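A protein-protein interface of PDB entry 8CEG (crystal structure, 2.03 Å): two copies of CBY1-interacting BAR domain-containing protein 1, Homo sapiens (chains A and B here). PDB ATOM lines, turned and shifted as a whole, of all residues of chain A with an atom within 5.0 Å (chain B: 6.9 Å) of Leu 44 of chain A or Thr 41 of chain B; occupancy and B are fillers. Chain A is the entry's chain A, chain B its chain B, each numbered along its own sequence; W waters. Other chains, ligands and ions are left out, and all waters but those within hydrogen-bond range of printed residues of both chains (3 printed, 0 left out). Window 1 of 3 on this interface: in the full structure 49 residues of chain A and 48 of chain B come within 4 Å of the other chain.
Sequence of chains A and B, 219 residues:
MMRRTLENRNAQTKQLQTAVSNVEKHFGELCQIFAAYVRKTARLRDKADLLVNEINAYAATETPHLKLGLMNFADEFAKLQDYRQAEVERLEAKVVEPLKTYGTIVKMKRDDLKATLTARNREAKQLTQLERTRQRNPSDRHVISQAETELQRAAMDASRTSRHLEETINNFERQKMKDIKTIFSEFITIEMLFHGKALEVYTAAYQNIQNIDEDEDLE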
ATOM      1  N   LYS A  40      -5.811  -2.402  10.310  1.00  0.00           N
ATOM      2  CA  LYS A  40      -5.844  -0.990   9.956  1.00  0.00           C
ATOM      3  C   LYS A  40      -4.727  -0.625   8.987  1.00  0.00           C
ATOM      4  O   LYS A  40      -4.903   0.257   8.136  1.00  0.00           O
ATOM      5  CB  LYS A  40      -5.729  -0.134  11.222  1.00  0.00           C
ATOM      6  CG  LYS A  40      -7.003  -0.025  12.105  1.00  0.00           C
ATOM      7  CD  LYS A  40      -8.292  -0.369  11.352  1.00  0.00           C
ATOM      8  CE  LYS A  40      -9.509  -0.289  12.245  1.00  0.00           C
ATOM      9  NZ  LYS A  40     -10.705  -0.789  11.531  1.00  0.00           N
ATOM     10  N   THR A  41      -3.555  -1.247   9.143  1.00  0.00           N
ATOM     11  CA  THR A  41      -2.445  -1.039   8.213  1.00  0.00           C
ATOM     12  C   THR A  41      -2.828  -1.529   6.806  1.00  0.00           C
ATOM     13  O   THR A  41      -2.619  -0.814   5.801  1.00  0.00           O
ATOM     14  CB  THR A  41      -1.193  -1.760   8.745  1.00  0.00           C
ATOM     15  OG1 THR A  41      -0.735  -1.191   9.994  1.00  0.00           O
ATOM     16  CG2 THR A  41      -0.030  -1.697   7.787  1.00  0.00           C
ATOM     17  N   ALA A  42      -3.509  -2.678   6.736  1.00  0.00           N
ATOM     18  CA  ALA A  42      -3.985  -3.192   5.461  1.00  0.00           C
ATOM     19  C   ALA A  42      -5.060  -2.294   4.855  1.00  0.00           C
ATOM     20  O   ALA A  42      -5.093  -2.117   3.638  1.00  0.00           O
ATOM     21  CB  ALA A  42      -4.538  -4.610   5.618  1.00  0.00           C
ATOM     22  N   ARG A  43      -5.962  -1.738   5.681  1.00  0.00           N
ATOM     23  CA  ARG A  43      -6.985  -0.840   5.140  1.00  0.00           C
ATOM     24  C   ARG A  43      -6.375   0.460   4.609  1.00  0.00           C
ATOM     25  O   ARG A  43      -6.852   0.996   3.604  1.00  0.00           O
ATOM     26  CB  ARG A  43      -8.081  -0.552   6.174  1.00  0.00           C
ATOM     27  CG  ARG A  43      -9.195  -1.656   6.296  1.00  0.00           C
ATOM     28  CD  ARG A  43     -10.213  -1.283   7.416  1.00  0.00           C
ATOM     29  NE  ARG A  43     -11.486  -0.724   6.947  1.00  0.00           N
ATOM     30  CZ  ARG A  43     -12.444  -0.254   7.746  1.00  0.00           C
ATOM     31  NH1 ARG A  43     -12.298  -0.245   9.067  1.00  0.00           N
ATOM     32  NH2 ARG A  43     -13.571   0.223   7.210  1.00  0.00           N
ATOM     33  N   LEU A  44      -5.343   0.984   5.279  1.00  0.00           N
ATOM     34  CA  LEU A  44      -4.580   2.108   4.747  1.00  0.00           C
ATOM     35  C   LEU A  44      -3.963   1.753   3.393  1.00  0.00           C
ATOM     36  O   LEU A  44      -4.026   2.545   2.432  1.00  0.00           O
ATOM     37  CB  LEU A  44      -3.500   2.519   5.769  1.00  0.00           C
ATOM     38  CG  LEU A  44      -2.516   3.645   5.413  1.00  0.00           C
ATOM     39  CD1 LEU A  44      -3.269   4.985   4.938  1.00  0.00           C
ATOM     40  CD2 LEU A  44      -1.576   3.911   6.571  1.00  0.00           C
ATOM     41  N   ARG A  45      -3.432   0.540   3.271  1.00  0.00           N
ATOM     42  CA  ARG A  45      -2.789   0.083   2.017  1.00  0.00           C
ATOM     43  C   ARG A  45      -3.846  -0.019   0.910  1.00  0.00           C
ATOM     44  O   ARG A  45      -3.484   0.216  -0.230  1.00  0.00           O
ATOM     45  CB  ARG A  45      -2.068  -1.247   2.223  1.00  0.00           C
ATOM     46  CG  ARG A  45      -1.163  -1.651   1.072  1.00  0.00           C
ATOM     47  CD  ARG A  45      -1.386  -3.081   0.623  1.00  0.00           C
ATOM     48  NE  ARG A  45      -2.798  -3.385   0.435  1.00  0.00           N
ATOM     49  CZ  ARG A  45      -3.494  -4.248   1.165  1.00  0.00           C
ATOM     50  NH1 ARG A  45      -3.274  -4.372   2.460  1.00  0.00           N
ATOM     51  NH2 ARG A  45      -4.436  -4.976   0.601  1.00  0.00           N
ATOM     52  N   ASP A  46      -5.083  -0.382   1.232  1.00  0.00           N
ATOM     53  CA  ASP A  46      -6.152  -0.400   0.233  1.00  0.00           C
ATOM     54  C   ASP A  46      -6.403   0.988  -0.341  1.00  0.00           C
ATOM     55  O   ASP A  46      -6.613   1.146  -1.557  1.00  0.00           O
ATOM     56  CB  ASP A  46      -7.467  -0.913   0.840  1.00  0.00           C
ATOM     57  CG  ASP A  46      -7.408  -2.395   1.222  1.00  0.00           C
ATOM     58  OD1 ASP A  46      -6.402  -3.067   0.848  1.00  0.00           O
ATOM     59  OD2 ASP A  46      -8.395  -2.870   1.853  1.00  0.00           O
ATOM     60  N   LYS A  47      -6.459   1.992   0.536  1.00  0.00           N
ATOM     61  CA  LYS A  47      -6.713   3.363   0.094  1.00  0.00           C
ATOM     62  C   LYS A  47      -5.538   3.908  -0.703  1.00  0.00           C
ATOM     63  O   LYS A  47      -5.731   4.614  -1.706  1.00  0.00           O
ATOM     64  CB  LYS A  47      -7.002   4.271   1.292  1.00  0.00           C
ATOM     65  CG  LYS A  47      -8.253   3.913   2.118  1.00  0.00           C
ATOM     66  CD  LYS A  47      -9.501   3.635   1.316  1.00  0.00           C
ATOM     67  CE  LYS A  47     -10.579   3.070   2.189  1.00  0.00           C
ATOM     68  NZ  LYS A  47     -11.883   3.293   1.572  1.00  0.00           N
ATOM     69  N   ALA A  48      -4.313   3.561  -0.304  1.00  0.00           N
ATOM     70  CA  ALA A  48      -3.163   3.984  -1.082  1.00  0.00           C
ATOM     71  C   ALA A  48      -3.204   3.371  -2.481  1.00  0.00           C
ATOM     72  O   ALA A  48      -2.818   4.020  -3.457  1.00  0.00           O
ATOM     73  CB  ALA A  48      -1.868   3.628  -0.385  1.00  0.00           C
ATOM     74  N   ARG A  84       4.423  -2.115   2.135  1.00  0.00           N
ATOM     75  CA  ARG A  84       3.454  -2.101   3.216  1.00  0.00           C
ATOM     76  C   ARG A  84       2.764  -3.453   3.349  1.00  0.00           C
ATOM     77  O   ARG A  84       2.455  -3.890   4.466  1.00  0.00           O
ATOM     78  CB  ARG A  84       2.405  -0.989   3.014  1.00  0.00           C
ATOM     79  CG  ARG A  84       1.463  -0.861   4.253  1.00  0.00           C
ATOM     80  CD  ARG A  84       0.576   0.351   4.271  1.00  0.00           C
ATOM     81  NE  ARG A  84       1.212   1.491   4.918  1.00  0.00           N
ATOM     82  CZ  ARG A  84       1.374   2.697   4.377  1.00  0.00           C
ATOM     83  NH1 ARG A  84       1.008   2.957   3.132  1.00  0.00           N
ATOM     84  NH2 ARG A  84       1.919   3.662   5.104  1.00  0.00           N
ATOM     85  N   ALA B  36      -9.850   9.741   2.400  1.00  0.00           N
ATOM     86  CA  ALA B  36      -9.995   8.403   2.976  1.00  0.00           C
ATOM     87  C   ALA B  36      -8.653   7.904   3.498  1.00  0.00           C
ATOM     88  O   ALA B  36      -8.577   7.291   4.572  1.00  0.00           O
ATOM     89  CB  ALA B  36     -10.553   7.413   1.955  1.00  0.00           C
ATOM     90  N   TYR B  37      -7.576   8.190   2.757  1.00  0.00           N
ATOM     91  CA  TYR B  37      -6.250   7.853   3.254  1.00  0.00           C
ATOM     92  C   TYR B  37      -5.975   8.501   4.611  1.00  0.00           C
ATOM     93  O   TYR B  37      -5.441   7.856   5.524  1.00  0.00           O
ATOM     94  CB  TYR B  37      -5.236   8.292   2.222  1.00  0.00           C
ATOM     95  CG  TYR B  37      -3.762   8.002   2.481  1.00  0.00           C
ATOM     96  CD1 TYR B  37      -2.983   8.873   3.215  1.00  0.00           C
ATOM     97  CD2 TYR B  37      -3.155   6.850   1.952  1.00  0.00           C
ATOM     98  CE1 TYR B  37      -1.635   8.621   3.437  1.00  0.00           C
ATOM     99  CE2 TYR B  37      -1.819   6.575   2.174  1.00  0.00           C
ATOM    100  CZ  TYR B  37      -1.053   7.493   2.890  1.00  0.00           C
ATOM    101  OH  TYR B  37       0.282   7.284   3.057  1.00  0.00           O
ATOM    102  N   VAL B  38      -6.333   9.769   4.772  1.00  0.00           N
ATOM    103  CA  VAL B  38      -6.134  10.426   6.057  1.00  0.00           C
ATOM    104  C   VAL B  38      -6.961   9.734   7.136  1.00  0.00           C
ATOM    105  O   VAL B  38      -6.470   9.475   8.232  1.00  0.00           O
ATOM    106  CB  VAL B  38      -6.469  11.920   5.949  1.00  0.00           C
ATOM    107  CG1 VAL B  38      -6.599  12.524   7.288  1.00  0.00           C
ATOM    108  CG2 VAL B  38      -5.376  12.716   5.112  1.00  0.00           C
ATOM    109  N   ARG B  39      -8.204   9.375   6.826  1.00  0.00           N
ATOM    110  CA  ARG B  39      -9.046   8.712   7.813  1.00  0.00           C
ATOM    111  C   ARG B  39      -8.470   7.371   8.240  1.00  0.00           C
ATOM    112  O   ARG B  39      -8.533   7.004   9.421  1.00  0.00           O
ATOM    113  CB  ARG B  39     -10.455   8.504   7.242  1.00  0.00           C
ATOM    114  CG  ARG B  39     -11.336   9.711   7.275  1.00  0.00           C
ATOM    115  CD  ARG B  39     -12.829   9.304   7.073  1.00  0.00           C
ATOM    116  NE  ARG B  39     -13.094   8.544   5.847  1.00  0.00           N
ATOM    117  CZ  ARG B  39     -13.301   9.092   4.649  1.00  0.00           C
ATOM    118  NH1 ARG B  39     -13.190  10.396   4.453  1.00  0.00           N
ATOM    119  NH2 ARG B  39     -13.622   8.311   3.618  1.00  0.00           N
ATOM    120  N   LYS B  40      -7.976   6.582   7.290  1.00  0.00           N
ATOM    121  CA  LYS B  40      -7.387   5.303   7.672  1.00  0.00           C
ATOM    122  C   LYS B  40      -6.115   5.501   8.483  1.00  0.00           C
ATOM    123  O   LYS B  40      -5.784   4.671   9.346  1.00  0.00           O
ATOM    124  CB  LYS B  40      -7.100   4.454   6.435  1.00  0.00           C
ATOM    125  CG  LYS B  40      -8.319   3.787   5.784  1.00  0.00           C
ATOM    126  CD  LYS B  40      -9.477   3.707   6.733  1.00  0.00           C
ATOM    127  CE  LYS B  40     -10.694   3.047   6.127  1.00  0.00           C
ATOM    128  NZ  LYS B  40     -11.869   3.161   7.051  1.00  0.00           N
ATOM    129  N   THR B  41      -5.365   6.552   8.185  1.00  0.00           N
ATOM    130  CA  THR B  41      -4.174   6.843   8.960  1.00  0.00           C
ATOM    131  C   THR B  41      -4.560   7.180  10.398  1.00  0.00           C
ATOM    132  O   THR B  41      -3.870   6.786  11.341  1.00  0.00           O
ATOM    133  CB  THR B  41      -3.381   7.981   8.321  1.00  0.00           C
ATOM    134  OG1 THR B  41      -2.874   7.616   7.022  1.00  0.00           O
ATOM    135  CG2 THR B  41      -2.210   8.362   9.185  1.00  0.00           C
ATOM    136  N   ALA B  42      -5.661   7.911  10.581  1.00  0.00           N
ATOM    137  CA  ALA B  42      -6.169   8.205  11.926  1.00  0.00           C
ATOM    138  C   ALA B  42      -6.709   6.955  12.612  1.00  0.00           C
ATOM    139  O   ALA B  42      -6.546   6.798  13.832  1.00  0.00           O
ATOM    140  CB  ALA B  42      -7.253   9.312  11.846  1.00  0.00           C
ATOM    141  N   ARG B  43      -7.365   6.051  11.861  1.00  0.00           N
ATOM    142  CA  ARG B  43      -7.845   4.807  12.465  1.00  0.00           C
ATOM    143  C   ARG B  43      -6.669   3.934  12.938  1.00  0.00           C
ATOM    144  O   ARG B  43      -6.758   3.267  13.987  1.00  0.00           O
ATOM    145  CB  ARG B  43      -8.699   3.994  11.481  1.00  0.00           C
ATOM    146  CG  ARG B  43     -10.141   4.464  11.220  1.00  0.00           C
ATOM    147  CD  ARG B  43     -11.081   4.415  12.411  1.00  0.00           C
ATOM    148  NE  ARG B  43     -11.551   3.065  12.744  1.00  0.00           N
ATOM    149  CZ  ARG B  43     -11.457   2.482  13.942  1.00  0.00           C
ATOM    150  NH1 ARG B  43     -10.927   3.110  14.984  1.00  0.00           N
ATOM    151  NH2 ARG B  43     -11.914   1.239  14.100  1.00  0.00           N
ATOM    152  N   LEU B  44      -5.573   3.887  12.150  1.00  0.00           N
ATOM    153  CA  LEU B  44      -4.346   3.210  12.595  1.00  0.00           C
ATOM    154  C   LEU B  44      -3.789   3.864  13.854  1.00  0.00           C
ATOM    155  O   LEU B  44      -3.406   3.183  14.807  1.00  0.00           O
ATOM    156  CB  LEU B  44      -3.313   3.227  11.466  1.00  0.00           C
ATOM    157  CG  LEU B  44      -1.904   2.667  11.683  1.00  0.00           C
ATOM    158  CD1 LEU B  44      -1.941   1.239  12.196  1.00  0.00           C
ATOM    159  CD2 LEU B  44      -1.087   2.725  10.401  1.00  0.00           C
ATOM    160  N   ARG B  45      -3.768   5.190  13.888  1.00  0.00           N
ATOM    161  CA  ARG B  45      -3.328   5.896  15.083  1.00  0.00           C
ATOM    162  C   ARG B  45      -4.190   5.517  16.294  1.00  0.00           C
ATOM    163  O   ARG B  45      -3.670   5.357  17.406  1.00  0.00           O
ATOM    164  CB  ARG B  45      -3.346   7.410  14.784  1.00  0.00           C
ATOM    165  CG  ARG B  45      -2.500   8.253  15.755  1.00  0.00           C
ATOM    166  CD  ARG B  45      -3.312   8.871  16.896  1.00  0.00           C
ATOM    167  NE  ARG B  45      -4.443   9.640  16.355  1.00  0.00           N
ATOM    168  CZ  ARG B  45      -5.714   9.399  16.654  1.00  0.00           C
ATOM    169  NH1 ARG B  45      -6.050   8.514  17.587  1.00  0.00           N
ATOM    170  NH2 ARG B  45      -6.671  10.029  15.989  1.00  0.00           N
ATOM    171  N   ASP B  46      -5.507   5.313  16.095  1.00  0.00           N
ATOM    172  CA  ASP B  46      -6.371   4.877  17.206  1.00  0.00           C
ATOM    173  C   ASP B  46      -5.928   3.536  17.780  1.00  0.00           C
ATOM    174  O   ASP B  46      -5.989   3.310  18.985  1.00  0.00           O
ATOM    175  CB  ASP B  46      -7.812   4.689  16.744  1.00  0.00           C
ATOM    176  CG  ASP B  46      -8.567   6.000  16.480  1.00  0.00           C
ATOM    177  OD1 ASP B  46      -8.127   7.089  16.927  1.00  0.00           O
ATOM    178  OD2 ASP B  46      -9.608   5.909  15.771  1.00  0.00           O
ATOM    179  N   GLN B  81       2.815   8.339  18.092  1.00  0.00           N
ATOM    180  CA  GLN B  81       1.417   8.509  17.698  1.00  0.00           C
ATOM    181  C   GLN B  81       1.016   9.976  17.701  1.00  0.00           C
ATOM    182  O   GLN B  81       0.160  10.381  16.899  1.00  0.00           O
ATOM    183  CB  GLN B  81       0.491   7.694  18.585  1.00  0.00           C
ATOM    184  CG  GLN B  81       0.748   6.175  18.551  1.00  0.00           C
ATOM    185  CD  GLN B  81       1.111   5.612  17.191  1.00  0.00           C
ATOM    186  OE1 GLN B  81       0.409   5.826  16.180  1.00  0.00           O
ATOM    187  NE2 GLN B  81       2.220   4.854  17.154  1.00  0.00           N
ATOM    188  N   ARG B  84       2.138  10.904  14.276  1.00  0.00           N
ATOM    189  CA  ARG B  84       1.132  10.450  13.333  1.00  0.00           C
ATOM    190  C   ARG B  84      -0.078  11.370  13.361  1.00  0.00           C
ATOM    191  O   ARG B  84      -0.629  11.687  12.308  1.00  0.00           O
ATOM    192  CB  ARG B  84       0.713   9.015  13.606  1.00  0.00           C
ATOM    193  CG  ARG B  84      -0.292   8.457  12.606  1.00  0.00           C
ATOM    194  CD  ARG B  84      -0.471   6.908  12.764  1.00  0.00           C
ATOM    195  NE  ARG B  84       0.469   6.169  11.920  1.00  0.00           N
ATOM    196  CZ  ARG B  84       1.302   5.213  12.328  1.00  0.00           C
ATOM    197  NH1 ARG B  84       1.383   4.858  13.596  1.00  0.00           N
ATOM    198  NH2 ARG B  84       2.063   4.593  11.440  1.00  0.00           N
ATOM    199  N   GLN B  85      -0.483  11.848  14.544  1.00  0.00           N
ATOM    200  CA  GLN B  85      -1.650  12.723  14.573  1.00  0.00           C
ATOM    201  C   GLN B  85      -1.335  14.039  13.855  1.00  0.00           C
ATOM    202  O   GLN B  85      -2.164  14.574  13.117  1.00  0.00           O
ATOM    203  CB  GLN B  85      -2.105  12.944  16.015  1.00  0.00           C
ATOM    204  CG  GLN B  85      -3.458  13.654  16.156  1.00  0.00           C
ATOM    205  CD  GLN B  85      -4.591  13.035  15.296  1.00  0.00           C
ATOM    206  OE1 GLN B  85      -4.660  11.814  15.084  1.00  0.00           O
ATOM    207  NE2 GLN B  85      -5.460  13.896  14.769  1.00  0.00           N
ATOM    208  N   GLU B  87       0.799  14.276  11.399  1.00  0.00           N
ATOM    209  CA  GLU B  87       0.768  13.911   9.986  1.00  0.00           C
ATOM    210  C   GLU B  87      -0.658  13.991   9.451  1.00  0.00           C
ATOM    211  O   GLU B  87      -0.916  14.637   8.431  1.00  0.00           O
ATOM    212  CB  GLU B  87       1.360  12.505   9.794  1.00  0.00           C
ATOM    213  CG  GLU B  87       1.245  11.937   8.386  1.00  0.00           C
ATOM    214  CD  GLU B  87       1.304  10.404   8.337  1.00  0.00           C
ATOM    215  OE1 GLU B  87       1.200   9.732   9.399  1.00  0.00           O
ATOM    216  OE2 GLU B  87       1.380   9.850   7.216  1.00  0.00           O
ATOM    217  N   VAL B  88      -1.595  13.361  10.167  1.00  0.00           N
ATOM    218  CA  VAL B  88      -3.021  13.403   9.830  1.00  0.00           C
ATOM    219  C   VAL B  88      -3.513  14.832   9.628  1.00  0.00           C
ATOM    220  O   VAL B  88      -4.205  15.139   8.639  1.00  0.00           O
ATOM    221  CB  VAL B  88      -3.827  12.704  10.939  1.00  0.00           C
ATOM    222  CG1 VAL B  88      -5.338  13.090  10.936  1.00  0.00           C
ATOM    223  CG2 VAL B  88      -3.662  11.254  10.806  1.00  0.00           C
ATOM    224  N   LEU B  91      -1.812  16.550   6.513  1.00  0.00           N
ATOM    225  CA  LEU B  91      -2.387  16.044   5.264  1.00  0.00           C
ATOM    226  C   LEU B  91      -3.755  16.679   4.987  1.00  0.00           C
ATOM    227  O   LEU B  91      -4.054  17.067   3.852  1.00  0.00           O
ATOM    228  CB  LEU B  91      -2.505  14.515   5.278  1.00  0.00           C
ATOM    229  CG  LEU B  91      -1.205  13.714   5.218  1.00  0.00           C
ATOM    230  CD1 LEU B  91      -1.441  12.198   5.356  1.00  0.00           C
ATOM    231  CD2 LEU B  91      -0.441  13.989   3.976  1.00  0.00           C
ATOM    232  N   GLU B 191       4.792  13.030   4.510  1.00  0.00           N
ATOM    233  CA  GLU B 191       5.044  11.619   4.797  1.00  0.00           C
ATOM    234  C   GLU B 191       6.499  11.378   5.129  1.00  0.00           C
ATOM    235  O   GLU B 191       6.821  10.662   6.076  1.00  0.00           O
ATOM    236  CB  GLU B 191       4.645  10.764   3.606  1.00  0.00           C
ATOM    237  CG  GLU B 191       3.183  10.805   3.294  1.00  0.00           C
ATOM    238  CD  GLU B 191       2.334  10.189   4.385  1.00  0.00           C
ATOM    239  OE1 GLU B 191       1.936  10.915   5.316  1.00  0.00           O
ATOM    240  OE2 GLU B 191       2.043   8.982   4.309  1.00  0.00           O
ATOM    241  N   PHE B 194       7.107  12.250   8.598  1.00  0.00           N
ATOM    242  CA  PHE B 194       6.646  11.235   9.522  1.00  0.00           C
ATOM    243  C   PHE B 194       7.561  10.002   9.498  1.00  0.00           C
ATOM    244  O   PHE B 194       7.925   9.456  10.549  1.00  0.00           O
ATOM    245  CB  PHE B 194       5.206  10.806   9.224  1.00  0.00           C
ATOM    246  CG  PHE B 194       4.770   9.682  10.144  1.00  0.00           C
ATOM    247  CD1 PHE B 194       4.582   9.928  11.485  1.00  0.00           C
ATOM    248  CD2 PHE B 194       4.688   8.363   9.693  1.00  0.00           C
ATOM    249  CE1 PHE B 194       4.244   8.894  12.358  1.00  0.00           C
ATOM    250  CE2 PHE B 194       4.356   7.370  10.521  1.00  0.00           C
ATOM    251  CZ  PHE B 194       4.139   7.614  11.871  1.00  0.00           C
HETATM  252  O   HOH W   1      -6.852   2.212   8.885  1.00  0.00           O
HETATM  253  O   HOH W   2       1.789   5.403   2.059  1.00  0.00           O
HETATM  254  O   HOH W   3       3.039   4.568   8.088  1.00  0.00           O
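Water W2 lies within hydrogen-bond range of the side-chain hydroxyl (OH) of Tyr 37 of chain B (2.6 Å) and the guanidinium group (NH1) of Arg 84 of chain A (2.8 Å).
Water W1 bridges O of Lys 40 of chain B and O of Lys 40 of chain A.
Water W3 bridges NH2 of Arg 84 of chain A (3.3 Å) and NH2 of Arg 84 of chain B (3.5 Å).
Lys 40 of chain A touches Leu 44 of chain B.
Thr 41 of chain A touches Leu 44 of chain B (OG1 to CD1, 3.5 Å).
Leu 44 of chain A touches Tyr 37 of chain B (CD1 to CE2, 3.5 Å).
CA of Leu 44 of chain A touches CB of Lys 40 of chain B (3.8 Å).
Leu 44 of chain A touches Thr 41 of chain B (CD1 to OG1, 3.4 Å).
CB of Ala 36 of chain B touches CD of Lys 47 of chain A, at 3.97 Å.
CG of Lys 47 of chain A touches CG of Lys 40 of chain B (3.7 Å).
CE2 of Tyr 37 of chain B touches CB of Ala 48 of chain A, at 3.9 Å.
Lys 40 of chain A touches Arg 43 of chain B, and with the chains exchanged Arg 43 of chain A touches Lys 40 of chain B.
Lys 40 of chain A touches Leu 44 of chain B, and with the chains exchanged Leu 44 of chain A touches Lys 40 of chain B.
Thr 41 of chain A touches Leu 44 of chain B, and with the chains exchanged Leu 44 of chain A touches Thr 41 of chain B.
Hydrophobic or aromatic side chains of chain A within 4 Å of the printed part of chain B: Leu 44 and Ala 48.
Along chain A the printed residues that touch a printed residue of chain B span positions 40 to 48.
Of the 19 printed residues of chain B, 6 touch a printed residue of chain A.
Hydrophobic or aromatic side chains of chain B that line the printed part of chain A: Ala 36, Tyr 37 and Leu 44.
OH of Tyr 37 of chain B sits at hydrogen-bond distance from OE2 of Glu 191 of chain B (2.7 Å).
OG1 of Thr 41 of chain B lies within hydrogen-bond range of O of Tyr 37 of chain B, at 3.0 Å.
NH1 of Arg 43 of chain B is in salt-bridge range of OD2 of Asp 46 of chain B (3.2 Å).
Leu 44 of chain A touches just these residues of chain B: Tyr 37, Lys 40 and Thr 41.
Thr 41 of chain B touches just one residue of chain A: Leu 44 (3.4 Å).
Printed residues of chain B within 4 Å of Lys 40 of chain A: Arg 43 and Leu 44.
Of the printed residues of chain B, Thr 41 of chain A touches Leu 44.
Printed residues of chain A within 4 Å of Leu 44 of chain B: Lys 40 (3.9 Å) and Thr 41 (3.5 Å).
Val 88 of chain B touches none of the printed residues of chain A.
The nearest residue of chain B that does not touch Leu 44 of chain A is Leu 44 of chain B (4.04 Å).
The nearest printed residue of chain A that does not touch Thr 41 of chain B is Lys 40 of chain A (6.3 Å).
The side-chain amino group (NZ) of Lys 40 of chain A lies close to the guanidinium group (NH2) of Arg 43 of chain B (3.5 Å).
NH2 of Arg 43 of chain A lies close to NZ of Lys 40 of chain B (3.4 Å).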
